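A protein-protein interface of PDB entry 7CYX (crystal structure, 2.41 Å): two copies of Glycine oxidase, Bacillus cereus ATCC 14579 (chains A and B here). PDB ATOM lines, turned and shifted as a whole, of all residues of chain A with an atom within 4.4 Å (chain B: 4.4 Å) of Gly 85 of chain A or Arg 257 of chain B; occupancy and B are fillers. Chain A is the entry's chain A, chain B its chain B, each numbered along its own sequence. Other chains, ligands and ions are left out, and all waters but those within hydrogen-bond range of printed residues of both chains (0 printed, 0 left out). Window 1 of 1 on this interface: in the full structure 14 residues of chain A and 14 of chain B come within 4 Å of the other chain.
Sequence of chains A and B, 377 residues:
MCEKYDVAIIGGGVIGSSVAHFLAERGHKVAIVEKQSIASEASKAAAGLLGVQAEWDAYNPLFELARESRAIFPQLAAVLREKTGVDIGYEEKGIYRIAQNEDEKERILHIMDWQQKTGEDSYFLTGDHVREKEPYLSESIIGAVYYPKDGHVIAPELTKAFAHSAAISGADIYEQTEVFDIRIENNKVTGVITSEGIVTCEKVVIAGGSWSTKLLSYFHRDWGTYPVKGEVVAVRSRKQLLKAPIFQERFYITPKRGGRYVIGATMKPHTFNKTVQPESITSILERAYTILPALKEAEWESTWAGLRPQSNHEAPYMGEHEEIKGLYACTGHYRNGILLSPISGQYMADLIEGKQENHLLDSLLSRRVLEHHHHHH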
ATOM      1  N   LEU A  80     -38.753  22.194   3.454  1.00  0.00           N
ATOM      2  CA  LEU A  80     -37.882  21.431   2.569  1.00  0.00           C
ATOM      3  C   LEU A  80     -36.438  21.500   3.092  1.00  0.00           C
ATOM      4  O   LEU A  80     -35.772  20.473   3.234  1.00  0.00           O
ATOM      5  CB  LEU A  80     -37.995  21.986   1.144  1.00  0.00           C
ATOM      6  CG  LEU A  80     -39.288  21.673   0.383  1.00  0.00           C
ATOM      7  CD1 LEU A  80     -39.341  22.471  -0.909  1.00  0.00           C
ATOM      8  CD2 LEU A  80     -39.438  20.190   0.082  1.00  0.00           C
ATOM      9  N   ARG A  81     -35.967  22.718   3.378  1.00  0.00           N
ATOM     10  CA  ARG A  81     -34.640  22.911   3.969  1.00  0.00           C
ATOM     11  C   ARG A  81     -34.480  21.984   5.186  1.00  0.00           C
ATOM     12  O   ARG A  81     -33.530  21.198   5.221  1.00  0.00           O
ATOM     13  CB  ARG A  81     -34.394  24.386   4.307  1.00  0.00           C
ATOM     14  CG  ARG A  81     -33.195  24.639   5.210  1.00  0.00           C
ATOM     15  CD  ARG A  81     -31.872  24.027   4.746  1.00  0.00           C
ATOM     16  NE  ARG A  81     -31.252  23.142   5.741  1.00  0.00           N
ATOM     17  CZ  ARG A  81     -29.943  23.002   5.953  1.00  0.00           C
ATOM     18  NH1 ARG A  81     -29.088  23.877   5.450  1.00  0.00           N
ATOM     19  NH2 ARG A  81     -29.497  21.995   6.687  1.00  0.00           N
ATOM     20  N   LYS A  83     -36.072  19.321   6.125  1.00  0.00           N
ATOM     21  CA  LYS A  83     -36.209  17.912   5.885  1.00  0.00           C
ATOM     22  C   LYS A  83     -35.041  17.368   5.051  1.00  0.00           C
ATOM     23  O   LYS A  83     -34.632  16.236   5.253  1.00  0.00           O
ATOM     24  CB  LYS A  83     -37.540  17.655   5.185  1.00  0.00           C
ATOM     25  CG  LYS A  83     -37.953  16.198   5.080  1.00  0.00           C
ATOM     26  CD  LYS A  83     -39.165  16.011   4.203  1.00  0.00           C
ATOM     27  CE  LYS A  83     -39.615  14.574   4.072  1.00  0.00           C
ATOM     28  NZ  LYS A  83     -40.855  14.503   3.270  1.00  0.00           N
ATOM     29  N   THR A  84     -34.541  18.135   4.076  1.00  0.00           N
ATOM     30  CA  THR A  84     -33.679  17.534   3.043  1.00  0.00           C
ATOM     31  C   THR A  84     -32.279  18.125   3.050  1.00  0.00           C
ATOM     32  O   THR A  84     -31.380  17.559   2.401  1.00  0.00           O
ATOM     33  CB  THR A  84     -34.214  17.754   1.623  1.00  0.00           C
ATOM     34  OG1 THR A  84     -34.064  19.131   1.263  1.00  0.00           O
ATOM     35  CG2 THR A  84     -35.660  17.344   1.490  1.00  0.00           C
ATOM     36  N   GLY A  85     -32.134  19.284   3.692  1.00  0.00           N
ATOM     37  CA  GLY A  85     -30.888  20.027   3.753  1.00  0.00           C
ATOM     38  C   GLY A  85     -30.747  21.023   2.618  1.00  0.00           C
ATOM     39  O   GLY A  85     -29.938  21.952   2.712  1.00  0.00           O
ATOM     40  N   VAL A  86     -31.542  20.834   1.550  1.00  0.00           N
ATOM     41  CA  VAL A  86     -31.488  21.680   0.368  1.00  0.00           C
ATOM     42  C   VAL A  86     -32.287  22.948   0.646  1.00  0.00           C
ATOM     43  O   VAL A  86     -33.445  22.844   0.977  1.00  0.00           O
ATOM     44  CB  VAL A  86     -32.037  20.971  -0.878  1.00  0.00           C
ATOM     45  CG1 VAL A  86     -32.165  21.936  -2.043  1.00  0.00           C
ATOM     46  CG2 VAL A  86     -31.180  19.778  -1.270  1.00  0.00           C
ATOM     47  N   ASP A  87     -31.623  24.104   0.528  1.00  0.00           N
ATOM     48  CA  ASP A  87     -32.242  25.425   0.462  1.00  0.00           C
ATOM     49  C   ASP A  87     -32.558  25.761  -1.001  1.00  0.00           C
ATOM     50  O   ASP A  87     -31.675  25.642  -1.853  1.00  0.00           O
ATOM     51  CB  ASP A  87     -31.301  26.500   1.009  1.00  0.00           C
ATOM     52  CG  ASP A  87     -31.922  27.883   1.080  1.00  0.00           C
ATOM     53  OD1 ASP A  87     -32.615  28.151   2.077  1.00  0.00           O
ATOM     54  OD2 ASP A  87     -31.691  28.683   0.145  1.00  0.00           O
ATOM     55  N   ASP B  87     -26.958  29.047   1.922  1.00  0.00           N
ATOM     56  CA  ASP B  87     -27.138  28.113   3.054  1.00  0.00           C
ATOM     57  C   ASP B  87     -25.820  27.350   3.174  1.00  0.00           C
ATOM     58  O   ASP B  87     -25.348  26.849   2.164  1.00  0.00           O
ATOM     59  CB  ASP B  87     -28.343  27.212   2.825  1.00  0.00           C
ATOM     60  CG  ASP B  87     -28.605  26.268   3.971  1.00  0.00           C
ATOM     61  OD1 ASP B  87     -27.701  25.525   4.323  1.00  0.00           O
ATOM     62  OD2 ASP B  87     -29.706  26.293   4.489  1.00  0.00           O
ATOM     63  N   GLY B  89     -25.248  24.634   4.849  1.00  0.00           N
ATOM     64  CA  GLY B  89     -25.438  23.203   5.122  1.00  0.00           C
ATOM     65  C   GLY B  89     -25.218  22.890   6.578  1.00  0.00           C
ATOM     66  O   GLY B  89     -24.787  21.800   6.876  1.00  0.00           O
ATOM     67  N   ILE B 154     -21.022  22.492   4.978  1.00  0.00           N
ATOM     68  CA  ILE B 154     -20.459  22.398   3.648  1.00  0.00           C
ATOM     69  C   ILE B 154     -19.403  23.495   3.527  1.00  0.00           C
ATOM     70  O   ILE B 154     -19.729  24.669   3.399  1.00  0.00           O
ATOM     71  CB  ILE B 154     -21.565  22.523   2.582  1.00  0.00           C
ATOM     72  CG1 ILE B 154     -22.749  21.623   2.931  1.00  0.00           C
ATOM     73  CG2 ILE B 154     -21.021  22.235   1.189  1.00  0.00           C
ATOM     74  CD1 ILE B 154     -23.827  21.582   1.873  1.00  0.00           C
ATOM     75  N   GLU B 157     -19.295  26.083   0.850  1.00  0.00           N
ATOM     76  CA  GLU B 157     -20.453  26.975   0.950  1.00  0.00           C
ATOM     77  C   GLU B 157     -20.222  28.009   2.058  1.00  0.00           C
ATOM     78  O   GLU B 157     -20.404  29.213   1.827  1.00  0.00           O
ATOM     79  CB  GLU B 157     -21.742  26.175   1.135  1.00  0.00           C
ATOM     80  CG  GLU B 157     -22.214  25.507  -0.158  1.00  0.00           C
ATOM     81  CD  GLU B 157     -22.721  26.432  -1.266  1.00  0.00           C
ATOM     82  OE1 GLU B 157     -23.892  26.876  -1.186  1.00  0.00           O
ATOM     83  OE2 GLU B 157     -21.950  26.705  -2.219  1.00  0.00           O
ATOM     84  N   LYS B 256     -24.200  14.383   2.740  1.00  0.00           N
ATOM     85  CA  LYS B 256     -24.419  15.781   2.426  1.00  0.00           C
ATOM     86  C   LYS B 256     -25.784  15.870   1.734  1.00  0.00           C
ATOM     87  O   LYS B 256     -26.205  14.907   1.098  1.00  0.00           O
ATOM     88  CB  LYS B 256     -23.326  16.347   1.507  1.00  0.00           C
ATOM     89  CG  LYS B 256     -21.905  16.354   2.058  1.00  0.00           C
ATOM     90  CD  LYS B 256     -21.656  17.446   3.082  1.00  0.00           C
ATOM     91  CE  LYS B 256     -20.414  17.214   3.921  1.00  0.00           C
ATOM     92  NZ  LYS B 256     -20.399  18.027   5.163  1.00  0.00           N
ATOM     93  N   ARG B 257     -26.443  17.025   1.857  1.00  0.00           N
ATOM     94  CA  ARG B 257     -27.723  17.302   1.215  1.00  0.00           C
ATOM     95  C   ARG B 257     -27.660  16.833  -0.249  1.00  0.00           C
ATOM     96  O   ARG B 257     -26.646  17.045  -0.937  1.00  0.00           O
ATOM     97  CB  ARG B 257     -28.052  18.797   1.332  1.00  0.00           C
ATOM     98  CG  ARG B 257     -27.078  19.717   0.611  1.00  0.00           C
ATOM     99  CD  ARG B 257     -27.390  21.182   0.855  1.00  0.00           C
ATOM    100  NE  ARG B 257     -26.656  22.067  -0.046  1.00  0.00           N
ATOM    101  CZ  ARG B 257     -26.418  23.353   0.203  1.00  0.00           C
ATOM    102  NH1 ARG B 257     -26.754  23.872   1.376  1.00  0.00           N
ATOM    103  NH2 ARG B 257     -25.852  24.109  -0.725  1.00  0.00           N
ATOM    104  N   GLY B 258     -28.724  16.161  -0.698  1.00  0.00           N
ATOM    105  CA  GLY B 258     -28.894  15.806  -2.110  1.00  0.00           C
ATOM    106  C   GLY B 258     -28.404  14.403  -2.443  1.00  0.00           C
ATOM    107  O   GLY B 258     -28.001  14.138  -3.579  1.00  0.00           O
ATOM    108  N   GLY B 259     -28.452  13.510  -1.450  1.00  0.00           N
ATOM    109  CA  GLY B 259     -28.147  12.103  -1.624  1.00  0.00           C
ATOM    110  C   GLY B 259     -26.677  11.835  -1.912  1.00  0.00           C
ATOM    111  O   GLY B 259     -26.361  10.800  -2.478  1.00  0.00           O
ATOM    112  N   ARG B 260     -25.816  12.744  -1.472  1.00  0.00           N
ATOM    113  CA  ARG B 260     -24.357  12.659  -1.679  1.00  0.00           C
ATOM    114  C   ARG B 260     -23.692  12.043  -0.451  1.00  0.00           C
ATOM    115  O   ARG B 260     -24.182  12.267   0.646  1.00  0.00           O
ATOM    116  CB  ARG B 260     -23.828  14.075  -1.893  1.00  0.00           C
ATOM    117  CG  ARG B 260     -22.386  14.146  -2.366  1.00  0.00           C
ATOM    118  CD  ARG B 260     -21.897  15.567  -2.519  1.00  0.00           C
ATOM    119  NE  ARG B 260     -20.667  15.580  -3.271  1.00  0.00           N
ATOM    120  CZ  ARG B 260     -19.743  16.509  -3.173  1.00  0.00           C
ATOM    121  NH1 ARG B 260     -18.861  16.655  -4.138  1.00  0.00           N
ATOM    122  NH2 ARG B 260     -19.707  17.291  -2.116  1.00  0.00           N
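NH1 of Arg 81 of chain A is in salt-bridge range of OD1 of Asp 87 of chain B (2.4 Å).
The backbone carbonyl oxygen (O) of Leu 80 of chain A sits at hydrogen-bond distance from the side-chain hydroxyl (OG1) of Thr 84 of chain A (2.9 Å). The guanidinium group of Arg 81 of chain A lies close to the backbone carbonyl oxygen of Gly 85 of chain A, 3.5 Å away. The backbone carbonyl oxygen (O) of Val 86 of chain A sits close to the backbone NH (N) of Arg 81 of chain A (3.5 Å). OD1 of Asp 87 of chain B sits at hydrogen-bond distance from N of Gly 89 of chain B. The guanidinium group of Arg 257 of chain B lies within salt-bridge range of the side-chain carboxylate of Asp 87 of chain B (3.5 Å). The guanidinium group (NH2) of Arg 257 of chain B lies within salt-bridge range of the side-chain carboxylate (OE1) of Glu 157 of chain B, 3.4 Å away.
Gly 89 of chain B touches Arg 81 of chain A (CA to NH1, 3.7 Å). Thr 84 of chain A touches Arg 257 of chain B. O of Gly 85 of chain A touches CD of Arg 257 of chain B (3.2 Å). Asp 87 of chain B touches Asp 87 of chain A (CB to CB, 3.5 Å).
Of the printed residues of chain B, Arg 81 of chain A touches Asp 87 (2.4 Å) and Gly 89 (3.7 Å). Lys 83 of chain A touches none of the printed residues of chain B. Of the printed residues of chain B, Thr 84 of chain A touches Arg 257. Of the printed residues of chain B, Gly 85 of chain A touches Arg 257 (3.2 Å). Printed residues of chain B within 4 Å of Asp 87 of chain A: Asp 87. Of the printed residues of chain A, Asp 87 of chain B touches Arg 81 (2.4 Å) and Asp 87 (3.5 Å). Of the printed residues of chain A, Gly 89 of chain B touches Arg 81. Lys 256 of chain B touches none of the printed residues of chain A. Of the printed residues of chain A, Arg 257 of chain B touches Thr 84 (3.7 Å) and Gly 85 (3.2 Å). The nearest printed residue of chain A that does not touch Asp 87 of chain B is Gly 85 of chain A (4.5 Å).
Of the 9 printed residues of chain B, 3 touch a printed residue of chain A.
Asp 87 of chain A touches its own counterpart, Asp 87 of chain B. Position printed for both chains: 87.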
